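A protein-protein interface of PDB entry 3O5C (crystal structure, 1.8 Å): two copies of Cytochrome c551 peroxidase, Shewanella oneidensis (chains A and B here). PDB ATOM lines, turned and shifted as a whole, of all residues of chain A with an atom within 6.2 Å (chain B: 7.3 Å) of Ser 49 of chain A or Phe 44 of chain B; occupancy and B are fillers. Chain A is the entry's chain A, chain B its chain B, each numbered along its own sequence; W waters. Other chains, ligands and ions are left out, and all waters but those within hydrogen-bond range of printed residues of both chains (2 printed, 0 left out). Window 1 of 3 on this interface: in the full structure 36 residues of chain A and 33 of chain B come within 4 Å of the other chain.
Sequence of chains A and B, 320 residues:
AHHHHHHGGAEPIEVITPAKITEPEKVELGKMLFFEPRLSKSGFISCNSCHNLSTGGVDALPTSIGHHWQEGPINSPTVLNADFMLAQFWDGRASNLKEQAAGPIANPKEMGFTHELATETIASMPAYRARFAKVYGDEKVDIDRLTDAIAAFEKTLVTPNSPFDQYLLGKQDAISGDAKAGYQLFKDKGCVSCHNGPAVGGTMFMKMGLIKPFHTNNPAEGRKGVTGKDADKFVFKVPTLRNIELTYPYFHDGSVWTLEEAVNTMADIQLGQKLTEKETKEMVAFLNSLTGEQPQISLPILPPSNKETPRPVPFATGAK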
ATOM      1  N   PHE A  34     -35.234  22.207  24.801  1.00  0.00           N
ATOM      2  CA  PHE A  34     -34.054  21.560  24.194  1.00  0.00           C
ATOM      3  C   PHE A  34     -33.190  22.528  23.376  1.00  0.00           C
ATOM      4  O   PHE A  34     -31.967  22.340  23.268  1.00  0.00           O
ATOM      5  CB  PHE A  34     -34.519  20.395  23.311  1.00  0.00           C
ATOM      6  CG  PHE A  34     -33.408  19.526  22.752  1.00  0.00           C
ATOM      7  CD1 PHE A  34     -33.085  18.311  23.353  1.00  0.00           C
ATOM      8  CD2 PHE A  34     -32.724  19.896  21.587  1.00  0.00           C
ATOM      9  CE1 PHE A  34     -32.076  17.489  22.833  1.00  0.00           C
ATOM     10  CE2 PHE A  34     -31.725  19.086  21.050  1.00  0.00           C
ATOM     11  CZ  PHE A  34     -31.400  17.877  21.672  1.00  0.00           C
ATOM     12  N   PHE A  44     -26.024  30.938  25.924  1.00  0.00           N
ATOM     13  CA  PHE A  44     -25.452  30.660  24.601  1.00  0.00           C
ATOM     14  C   PHE A  44     -25.459  29.173  24.246  1.00  0.00           C
ATOM     15  O   PHE A  44     -25.324  28.830  23.069  1.00  0.00           O
ATOM     16  CB  PHE A  44     -24.012  31.213  24.546  1.00  0.00           C
ATOM     17  CG  PHE A  44     -23.383  31.195  23.174  1.00  0.00           C
ATOM     18  CD1 PHE A  44     -23.926  31.949  22.126  1.00  0.00           C
ATOM     19  CD2 PHE A  44     -22.237  30.442  22.928  1.00  0.00           C
ATOM     20  CE1 PHE A  44     -23.337  31.947  20.862  1.00  0.00           C
ATOM     21  CE2 PHE A  44     -21.639  30.437  21.667  1.00  0.00           C
ATOM     22  CZ  PHE A  44     -22.194  31.187  20.628  1.00  0.00           C
ATOM     23  N   ILE A  45     -25.630  28.304  25.246  1.00  0.00           N
ATOM     24  CA  ILE A  45     -25.594  26.842  25.038  1.00  0.00           C
ATOM     25  C   ILE A  45     -26.962  26.242  25.318  1.00  0.00           C
ATOM     26  O   ILE A  45     -27.574  26.540  26.339  1.00  0.00           O
ATOM     27  CB  ILE A  45     -24.561  26.171  25.983  1.00  0.00           C
ATOM     28  CG1 ILE A  45     -23.161  26.695  25.676  1.00  0.00           C
ATOM     29  CG2 ILE A  45     -24.639  24.625  25.907  1.00  0.00           C
ATOM     30  CD1 ILE A  45     -22.121  26.360  26.749  1.00  0.00           C
ATOM     31  N   SER A  46     -27.423  25.374  24.415  1.00  0.00           N
ATOM     32  CA  SER A  46     -28.654  24.646  24.593  1.00  0.00           C
ATOM     33  C   SER A  46     -28.323  23.161  24.437  1.00  0.00           C
ATOM     34  O   SER A  46     -27.176  22.804  24.132  1.00  0.00           O
ATOM     35  CB  SER A  46     -29.687  25.059  23.546  1.00  0.00           C
ATOM     36  OG  SER A  46     -29.337  24.521  22.280  1.00  0.00           O
ATOM     37  N   CYS A  47     -29.306  22.300  24.651  1.00  0.00           N
ATOM     38  CA  CYS A  47     -29.085  20.867  24.418  1.00  0.00           C
ATOM     39  C   CYS A  47     -28.637  20.642  22.979  1.00  0.00           C
ATOM     40  O   CYS A  47     -27.759  19.825  22.713  1.00  0.00           O
ATOM     41  CB  CYS A  47     -30.340  20.039  24.678  1.00  0.00           C
ATOM     42  SG  CYS A  47     -31.191  20.424  26.191  1.00  0.00           S
ATOM     43  N   ASN A  48     -29.252  21.373  22.049  1.00  0.00           N
ATOM     44  CA  ASN A  48     -28.978  21.183  20.627  1.00  0.00           C
ATOM     45  C   ASN A  48     -27.532  21.520  20.280  1.00  0.00           C
ATOM     46  O   ASN A  48     -26.964  20.909  19.363  1.00  0.00           O
ATOM     47  CB  ASN A  48     -29.977  21.978  19.768  1.00  0.00           C
ATOM     48  CG  ASN A  48     -29.909  21.629  18.297  1.00  0.00           C
ATOM     49  OD1 ASN A  48     -30.225  20.498  17.890  1.00  0.00           O
ATOM     50  ND2 ASN A  48     -29.543  22.607  17.476  1.00  0.00           N
ATOM     51  N   SER A  49     -26.931  22.467  21.004  1.00  0.00           N
ATOM     52  CA  SER A  49     -25.489  22.764  20.849  1.00  0.00           C
ATOM     53  C   SER A  49     -24.638  21.487  20.796  1.00  0.00           C
ATOM     54  O   SER A  49     -23.836  21.317  19.899  1.00  0.00           O
ATOM     55  CB  SER A  49     -24.981  23.661  21.976  1.00  0.00           C
ATOM     56  OG  SER A  49     -25.691  24.900  22.060  1.00  0.00           O
ATOM     57  N   CYS A  50     -24.826  20.592  21.756  1.00  0.00           N
ATOM     58  CA  CYS A  50     -23.993  19.394  21.836  1.00  0.00           C
ATOM     59  C   CYS A  50     -24.590  18.144  21.226  1.00  0.00           C
ATOM     60  O   CYS A  50     -23.880  17.149  21.044  1.00  0.00           O
ATOM     61  CB  CYS A  50     -23.620  19.144  23.276  1.00  0.00           C
ATOM     62  SG  CYS A  50     -22.775  20.540  23.968  1.00  0.00           S
ATOM     63  N   HIS A  51     -25.883  18.221  20.904  1.00  0.00           N
ATOM     64  CA  HIS A  51     -26.655  17.124  20.332  1.00  0.00           C
ATOM     65  C   HIS A  51     -27.395  17.649  19.113  1.00  0.00           C
ATOM     66  O   HIS A  51     -28.606  17.479  18.962  1.00  0.00           O
ATOM     67  CB  HIS A  51     -27.641  16.596  21.368  1.00  0.00           C
ATOM     68  CG  HIS A  51     -26.962  16.098  22.590  1.00  0.00           C
ATOM     69  ND1 HIS A  51     -26.276  14.902  22.620  1.00  0.00           N
ATOM     70  CD2 HIS A  51     -26.777  16.678  23.798  1.00  0.00           C
ATOM     71  CE1 HIS A  51     -25.740  14.745  23.816  1.00  0.00           C
ATOM     72  NE2 HIS A  51     -26.017  15.814  24.543  1.00  0.00           N
ATOM     73  N   ASN A  52     -26.623  18.296  18.250  1.00  0.00           N
ATOM     74  CA  ASN A  52     -27.149  19.057  17.149  1.00  0.00           C
ATOM     75  C   ASN A  52     -27.997  18.188  16.238  1.00  0.00           C
ATOM     76  O   ASN A  52     -27.501  17.281  15.610  1.00  0.00           O
ATOM     77  CB  ASN A  52     -25.984  19.692  16.386  1.00  0.00           C
ATOM     78  CG  ASN A  52     -26.419  20.809  15.466  1.00  0.00           C
ATOM     79  OD1 ASN A  52     -27.458  20.714  14.783  1.00  0.00           O
ATOM     80  ND2 ASN A  52     -25.610  21.884  15.418  1.00  0.00           N
ATOM     81  N   VAL A  58     -25.648  15.012  17.512  1.00  0.00           N
ATOM     82  CA  VAL A  58     -24.331  15.139  18.172  1.00  0.00           C
ATOM     83  C   VAL A  58     -23.583  16.390  17.678  1.00  0.00           C
ATOM     84  O   VAL A  58     -23.865  16.890  16.581  1.00  0.00           O
ATOM     85  CB  VAL A  58     -23.437  13.909  17.900  1.00  0.00           C
ATOM     86  CG1 VAL A  58     -24.038  12.635  18.503  1.00  0.00           C
ATOM     87  CG2 VAL A  58     -23.182  13.723  16.370  1.00  0.00           C
ATOM     88  N   ASP A  59     -22.615  16.882  18.463  1.00  0.00           N
ATOM     89  CA  ASP A  59     -21.745  17.990  18.017  1.00  0.00           C
ATOM     90  C   ASP A  59     -20.646  17.537  17.030  1.00  0.00           C
ATOM     91  O   ASP A  59     -19.994  18.380  16.404  1.00  0.00           O
ATOM     92  CB  ASP A  59     -21.132  18.785  19.193  1.00  0.00           C
ATOM     93  CG  ASP A  59     -20.498  17.898  20.269  1.00  0.00           C
ATOM     94  OD1 ASP A  59     -19.937  16.830  19.944  1.00  0.00           O
ATOM     95  OD2 ASP A  59     -20.559  18.289  21.456  1.00  0.00           O
ATOM     96  N   LEU A  61     -17.781  16.473  17.647  1.00  0.00           N
ATOM     97  CA  LEU A  61     -16.479  16.842  18.164  1.00  0.00           C
ATOM     98  C   LEU A  61     -15.968  15.684  19.016  1.00  0.00           C
ATOM     99  O   LEU A  61     -16.752  14.903  19.547  1.00  0.00           O
ATOM    100  CB  LEU A  61     -16.562  18.136  18.997  1.00  0.00           C
ATOM    101  CG  LEU A  61     -17.194  19.311  18.245  1.00  0.00           C
ATOM    102  CD1 LEU A  61     -17.329  20.556  19.118  1.00  0.00           C
ATOM    103  CD2 LEU A  61     -16.396  19.599  16.999  1.00  0.00           C
ATOM    104  N   ILE A  65     -17.762  21.116  23.786  1.00  0.00           N
ATOM    105  CA  ILE A  65     -17.459  22.478  24.164  1.00  0.00           C
ATOM    106  C   ILE A  65     -18.565  22.942  25.095  1.00  0.00           C
ATOM    107  O   ILE A  65     -19.745  22.922  24.714  1.00  0.00           O
ATOM    108  CB  ILE A  65     -17.433  23.409  22.914  1.00  0.00           C
ATOM    109  CG1 ILE A  65     -16.292  23.010  21.975  1.00  0.00           C
ATOM    110  CG2 ILE A  65     -17.311  24.850  23.334  1.00  0.00           C
ATOM    111  CD1 ILE A  65     -16.365  23.610  20.557  1.00  0.00           C
ATOM    112  N   GLY A  66     -18.189  23.347  26.308  1.00  0.00           N
ATOM    113  CA  GLY A  66     -19.142  23.838  27.312  1.00  0.00           C
ATOM    114  C   GLY A  66     -18.935  25.298  27.653  1.00  0.00           C
ATOM    115  O   GLY A  66     -18.220  26.004  26.966  1.00  0.00           O
ATOM    116  N   TRP A  69     -16.045  27.718  27.010  1.00  0.00           N
ATOM    117  CA  TRP A  69     -15.329  26.932  26.015  1.00  0.00           C
ATOM    118  C   TRP A  69     -14.421  25.893  26.691  1.00  0.00           C
ATOM    119  O   TRP A  69     -13.276  25.700  26.307  1.00  0.00           O
ATOM    120  CB  TRP A  69     -14.553  27.865  25.074  1.00  0.00           C
ATOM    121  CG  TRP A  69     -14.203  27.272  23.749  1.00  0.00           C
ATOM    122  CD1 TRP A  69     -13.158  26.436  23.468  1.00  0.00           C
ATOM    123  CD2 TRP A  69     -14.885  27.484  22.510  1.00  0.00           C
ATOM    124  NE1 TRP A  69     -13.158  26.102  22.139  1.00  0.00           N
ATOM    125  CE2 TRP A  69     -14.206  26.736  21.525  1.00  0.00           C
ATOM    126  CE3 TRP A  69     -16.005  28.237  22.131  1.00  0.00           C
ATOM    127  CZ2 TRP A  69     -14.612  26.713  20.187  1.00  0.00           C
ATOM    128  CZ3 TRP A  69     -16.405  28.213  20.801  1.00  0.00           C
ATOM    129  CH2 TRP A  69     -15.709  27.462  19.846  1.00  0.00           C
ATOM    130  N   GLU B  36     -24.804  25.613   9.309  1.00  0.00           N
ATOM    131  CA  GLU B  36     -23.697  24.706   9.122  1.00  0.00           C
ATOM    132  C   GLU B  36     -22.565  25.137  10.061  1.00  0.00           C
ATOM    133  O   GLU B  36     -21.933  26.165   9.820  1.00  0.00           O
ATOM    134  CB  GLU B  36     -23.277  24.749   7.659  1.00  0.00           C
ATOM    135  CG  GLU B  36     -22.087  23.883   7.309  1.00  0.00           C
ATOM    136  CD  GLU B  36     -22.258  22.488   7.784  1.00  0.00           C
ATOM    137  OE1 GLU B  36     -21.787  22.210   8.920  1.00  0.00           O
ATOM    138  OE2 GLU B  36     -22.867  21.686   7.031  1.00  0.00           O
ATOM    139  N   PRO B  37     -22.327  24.388  11.151  1.00  0.00           N
ATOM    140  CA  PRO B  37     -21.228  24.822  12.036  1.00  0.00           C
ATOM    141  C   PRO B  37     -19.831  24.503  11.485  1.00  0.00           C
ATOM    142  O   PRO B  37     -18.826  24.989  12.007  1.00  0.00           O
ATOM    143  CB  PRO B  37     -21.489  24.022  13.325  1.00  0.00           C
ATOM    144  CG  PRO B  37     -22.129  22.772  12.862  1.00  0.00           C
ATOM    145  CD  PRO B  37     -22.936  23.127  11.623  1.00  0.00           C
ATOM    146  N   ARG B  38     -19.751  23.667  10.449  1.00  0.00           N
ATOM    147  CA  ARG B  38     -18.469  23.387   9.817  1.00  0.00           C
ATOM    148  C   ARG B  38     -17.974  24.533   8.907  1.00  0.00           C
ATOM    149  O   ARG B  38     -16.900  24.421   8.290  1.00  0.00           O
ATOM    150  CB  ARG B  38     -18.505  22.047   9.093  1.00  0.00           C
ATOM    151  CG  ARG B  38     -18.752  20.870  10.049  1.00  0.00           C
ATOM    152  CD  ARG B  38     -19.162  19.619   9.315  1.00  0.00           C
ATOM    153  NE  ARG B  38     -20.514  19.730   8.756  1.00  0.00           N
ATOM    154  CZ  ARG B  38     -21.173  18.736   8.173  1.00  0.00           C
ATOM    155  NH1 ARG B  38     -20.629  17.534   8.070  1.00  0.00           N
ATOM    156  NH2 ARG B  38     -22.401  18.945   7.698  1.00  0.00           N
ATOM    157  N   LEU B  39     -18.739  25.629   8.840  1.00  0.00           N
ATOM    158  CA  LEU B  39     -18.234  26.915   8.320  1.00  0.00           C
ATOM    159  C   LEU B  39     -17.257  27.568   9.304  1.00  0.00           C
ATOM    160  O   LEU B  39     -16.606  28.539   8.957  1.00  0.00           O
ATOM    161  CB  LEU B  39     -19.360  27.897   7.983  1.00  0.00           C
ATOM    162  CG  LEU B  39     -20.018  27.657   6.621  1.00  0.00           C
ATOM    163  CD1 LEU B  39     -20.598  26.322   6.601  1.00  0.00           C
ATOM    164  CD2 LEU B  39     -21.079  28.690   6.290  1.00  0.00           C
ATOM    165  N   SER B  40     -17.169  27.044  10.529  1.00  0.00           N
ATOM    166  CA  SER B  40     -16.274  27.620  11.528  1.00  0.00           C
ATOM    167  C   SER B  40     -15.092  26.705  11.809  1.00  0.00           C
ATOM    168  O   SER B  40     -15.141  25.497  11.578  1.00  0.00           O
ATOM    169  CB  SER B  40     -17.023  27.913  12.817  1.00  0.00           C
ATOM    170  OG  SER B  40     -17.429  26.740  13.491  1.00  0.00           O
ATOM    171  N   LYS B  41     -14.018  27.304  12.296  1.00  0.00           N
ATOM    172  CA  LYS B  41     -12.826  26.555  12.657  1.00  0.00           C
ATOM    173  C   LYS B  41     -13.151  25.448  13.665  1.00  0.00           C
ATOM    174  O   LYS B  41     -12.682  24.333  13.525  1.00  0.00           O
ATOM    175  CB  LYS B  41     -11.821  27.538  13.250  1.00  0.00           C
ATOM    176  CG  LYS B  41     -10.558  26.932  13.816  1.00  0.00           C
ATOM    177  CD  LYS B  41      -9.700  26.342  12.733  1.00  0.00           C
ATOM    178  CE  LYS B  41      -8.226  26.328  13.179  1.00  0.00           C
ATOM    179  NZ  LYS B  41      -7.393  25.471  12.285  1.00  0.00           N
ATOM    180  N   SER B  42     -13.943  25.789  14.673  1.00  0.00           N
ATOM    181  CA  SER B  42     -14.294  24.874  15.782  1.00  0.00           C
ATOM    182  C   SER B  42     -15.200  23.709  15.398  1.00  0.00           C
ATOM    183  O   SER B  42     -15.203  22.683  16.083  1.00  0.00           O
ATOM    184  CB  SER B  42     -14.984  25.652  16.897  1.00  0.00           C
ATOM    185  OG  SER B  42     -16.201  26.231  16.437  1.00  0.00           O
ATOM    186  N   GLY B  43     -15.965  23.873  14.320  1.00  0.00           N
ATOM    187  CA  GLY B  43     -17.039  22.956  13.962  1.00  0.00           C
ATOM    188  C   GLY B  43     -18.216  23.092  14.916  1.00  0.00           C
ATOM    189  O   GLY B  43     -18.997  22.168  15.077  1.00  0.00           O
ATOM    190  N   PHE B  44     -18.332  24.254  15.555  1.00  0.00           N
ATOM    191  CA  PHE B  44     -19.316  24.471  16.612  1.00  0.00           C
ATOM    192  C   PHE B  44     -20.146  25.742  16.409  1.00  0.00           C
ATOM    193  O   PHE B  44     -21.241  25.845  16.952  1.00  0.00           O
ATOM    194  CB  PHE B  44     -18.571  24.493  17.963  1.00  0.00           C
ATOM    195  CG  PHE B  44     -19.458  24.572  19.169  1.00  0.00           C
ATOM    196  CD1 PHE B  44     -19.424  25.686  19.989  1.00  0.00           C
ATOM    197  CD2 PHE B  44     -20.294  23.510  19.516  1.00  0.00           C
ATOM    198  CE1 PHE B  44     -20.224  25.770  21.131  1.00  0.00           C
ATOM    199  CE2 PHE B  44     -21.097  23.579  20.662  1.00  0.00           C
ATOM    200  CZ  PHE B  44     -21.061  24.712  21.469  1.00  0.00           C
ATOM    201  N   ILE B  45     -19.641  26.710  15.642  1.00  0.00           N
ATOM    202  CA  ILE B  45     -20.332  27.989  15.472  1.00  0.00           C
ATOM    203  C   ILE B  45     -20.904  28.137  14.064  1.00  0.00           C
ATOM    204  O   ILE B  45     -20.147  28.097  13.092  1.00  0.00           O
ATOM    205  CB  ILE B  45     -19.381  29.173  15.719  1.00  0.00           C
ATOM    206  CG1 ILE B  45     -18.697  29.025  17.078  1.00  0.00           C
ATOM    207  CG2 ILE B  45     -20.131  30.505  15.642  1.00  0.00           C
ATOM    208  CD1 ILE B  45     -18.147  30.324  17.673  1.00  0.00           C
ATOM    209  N   SER B  46     -22.223  28.320  13.965  1.00  0.00           N
ATOM    210  CA  SER B  46     -22.893  28.589  12.691  1.00  0.00           C
ATOM    211  C   SER B  46     -23.440  30.014  12.716  1.00  0.00           C
ATOM    212  O   SER B  46     -23.441  30.669  13.766  1.00  0.00           O
ATOM    213  CB  SER B  46     -24.035  27.595  12.458  1.00  0.00           C
ATOM    214  OG  SER B  46     -25.087  27.762  13.426  1.00  0.00           O
ATOM    215  N   SER B  49     -25.737  30.536  15.522  1.00  0.00           N
ATOM    216  CA  SER B  49     -25.244  30.648  16.878  1.00  0.00           C
ATOM    217  C   SER B  49     -25.391  32.100  17.318  1.00  0.00           C
ATOM    218  O   SER B  49     -25.831  32.371  18.417  1.00  0.00           O
ATOM    219  CB  SER B  49     -23.787  30.161  17.011  1.00  0.00           C
ATOM    220  OG  SER B  49     -23.588  28.909  16.351  1.00  0.00           O
ATOM    221  N   GLY B  66     -17.616  34.281  20.467  1.00  0.00           N
ATOM    222  CA  GLY B  66     -17.084  33.708  19.241  1.00  0.00           C
ATOM    223  C   GLY B  66     -16.179  32.524  19.490  1.00  0.00           C
ATOM    224  O   GLY B  66     -16.206  31.923  20.563  1.00  0.00           O
ATOM    225  N   TRP B  69     -14.540  31.299  22.766  1.00  0.00           N
ATOM    226  CA  TRP B  69     -15.266  32.111  23.747  1.00  0.00           C
ATOM    227  C   TRP B  69     -14.734  33.547  23.791  1.00  0.00           C
ATOM    228  O   TRP B  69     -14.792  34.208  24.829  1.00  0.00           O
ATOM    229  CB  TRP B  69     -15.208  31.447  25.130  1.00  0.00           C
ATOM    230  CG  TRP B  69     -16.375  31.724  25.999  1.00  0.00           C
ATOM    231  CD1 TRP B  69     -16.500  32.739  26.916  1.00  0.00           C
ATOM    232  CD2 TRP B  69     -17.605  30.995  26.041  1.00  0.00           C
ATOM    233  NE1 TRP B  69     -17.731  32.677  27.531  1.00  0.00           N
ATOM    234  CE2 TRP B  69     -18.431  31.618  27.009  1.00  0.00           C
ATOM    235  CE3 TRP B  69     -18.087  29.863  25.373  1.00  0.00           C
ATOM    236  CZ2 TRP B  69     -19.711  31.147  27.319  1.00  0.00           C
ATOM    237  CZ3 TRP B  69     -19.367  29.400  25.680  1.00  0.00           C
ATOM    238  CH2 TRP B  69     -20.162  30.048  26.635  1.00  0.00           C
ATOM    239  N   PRO B 312     -12.514  19.565  12.414  1.00  0.00           N
ATOM    240  CA  PRO B 312     -12.627  20.745  13.245  1.00  0.00           C
ATOM    241  C   PRO B 312     -11.529  20.830  14.294  1.00  0.00           C
ATOM    242  O   PRO B 312     -10.971  19.813  14.690  1.00  0.00           O
ATOM    243  CB  PRO B 312     -13.983  20.553  13.931  1.00  0.00           C
ATOM    244  CG  PRO B 312     -14.165  19.139  13.990  1.00  0.00           C
ATOM    245  CD  PRO B 312     -13.580  18.598  12.731  1.00  0.00           C
ATOM    246  N   PRO B 314     -11.653  22.537  17.721  1.00  0.00           N
ATOM    247  CA  PRO B 314     -12.338  23.291  18.782  1.00  0.00           C
ATOM    248  C   PRO B 314     -11.373  23.798  19.846  1.00  0.00           C
ATOM    249  O   PRO B 314     -11.580  24.856  20.445  1.00  0.00           O
ATOM    250  CB  PRO B 314     -13.298  22.260  19.395  1.00  0.00           C
ATOM    251  CG  PRO B 314     -12.765  20.925  18.995  1.00  0.00           C
ATOM    252  CD  PRO B 314     -12.091  21.132  17.675  1.00  0.00           C
HETATM  253  O   HOH W   1     -21.163  21.002  16.357  1.00  0.00           O
HETATM  254  O   HOH W   2     -18.603  19.769  14.256  1.00  0.00           O
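Hydrophobic or aromatic side chains of chain B within 4 Å of the printed part of chain A: Phe 44, Trp 69, Pro 312 and Pro 314. Along chain B the printed residues that touch a printed residue of chain A span positions 42 to 314. Of the 16 printed residues of chain A, 6 touch a printed residue of chain B. Among the printed residues, 11 pairs touch across the chains.
The indole nitrogen of Trp 69 of chain A is in hydrogen-bond range of the backbone carbonyl oxygen of Pro 314 of chain B (2.6 Å).
Water W2 lies within hydrogen-bond range of O of Gly 43 of chain B and O of Asp 59 of chain A. Water W1 lies within hydrogen-bond range of the backbone carbonyl oxygen (O) of Gly 43 of chain B (2.8 Å) and the backbone carbonyl oxygen (O) of Asp 59 of chain A (2.9 Å).
Ser 49 of chain A touches one residue of chain B. Printed residues of chain A within 4 Å of Phe 44 of chain B: Ser 49 (3.6 Å) and Ile 65 (3.5 Å). Of the printed residues of chain B, Phe 44 of chain A touches Ser 49. Of the printed residues of chain A, Pro 312 of chain B touches Leu 61. Cys 50 of chain A touches none of the printed residues of chain B. His 51 of chain A touches none of the printed residues of chain B. The nearest printed residue of chain A that does not touch Phe 44 of chain B is Trp 69 of chain A (4.02 Å).
Ser 49 of chain B touches Phe 44 of chain A. Ser 49 of chain A touches Phe 44 of chain B. Leu 61 of chain A touches Ser 42 of chain B (CD2 to O, 3.4 Å). Leu 61 of chain A touches Pro 312 of chain B. Ile 65 of chain A touches Phe 44 of chain B. Ile 65 of chain A touches Pro 314 of chain B (CD1 to CB, 3.5 Å). O of Gly 66 of chain A touches CZ3 of Trp 69 of chain B, at 3.8 Å. Ser 42 of chain B touches Trp 69 of chain A. CZ3 of Trp 69 of chain A touches O of Gly 66 of chain B (3.7 Å). Trp 69 of chain A touches Trp 69 of chain B (N to CE3, 3.4 Å).
N of Ser 46 of chain A lies within hydrogen-bond range of OG of Ser 49 of chain A (3.0 Å). The backbone NH (N) of Leu 61 of chain A sits close to the side-chain carboxylate (OD1) of Asp 59 of chain A. The side-chain hydroxyl (OG) of Ser 40 of chain B is in hydrogen-bond range of the side-chain hydroxyl (OG) of Ser 42 of chain B, 3.2 Å away. OG of Ser 40 of chain B sits at hydrogen-bond distance from N of Phe 44 of chain B (3.4 Å). The side-chain hydroxyl of Ser 42 of chain B lies within hydrogen-bond range of the backbone NH of Phe 44 of chain B. The side-chain hydroxyl of Ser 49 of chain B lies within hydrogen-bond range of the backbone NH of Ser 46 of chain B (2.8 Å).
Phe 44 of chain A touches Ser 49 of chain B, and with the chains exchanged Ser 49 of chain A touches Phe 44 of chain B. Gly 66 of chain A touches Trp 69 of chain B, and with the chains exchanged Trp 69 of chain A touches Gly 66 of chain B. Trp 69 of chain B touches its own counterpart, Trp 69 of chain A.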
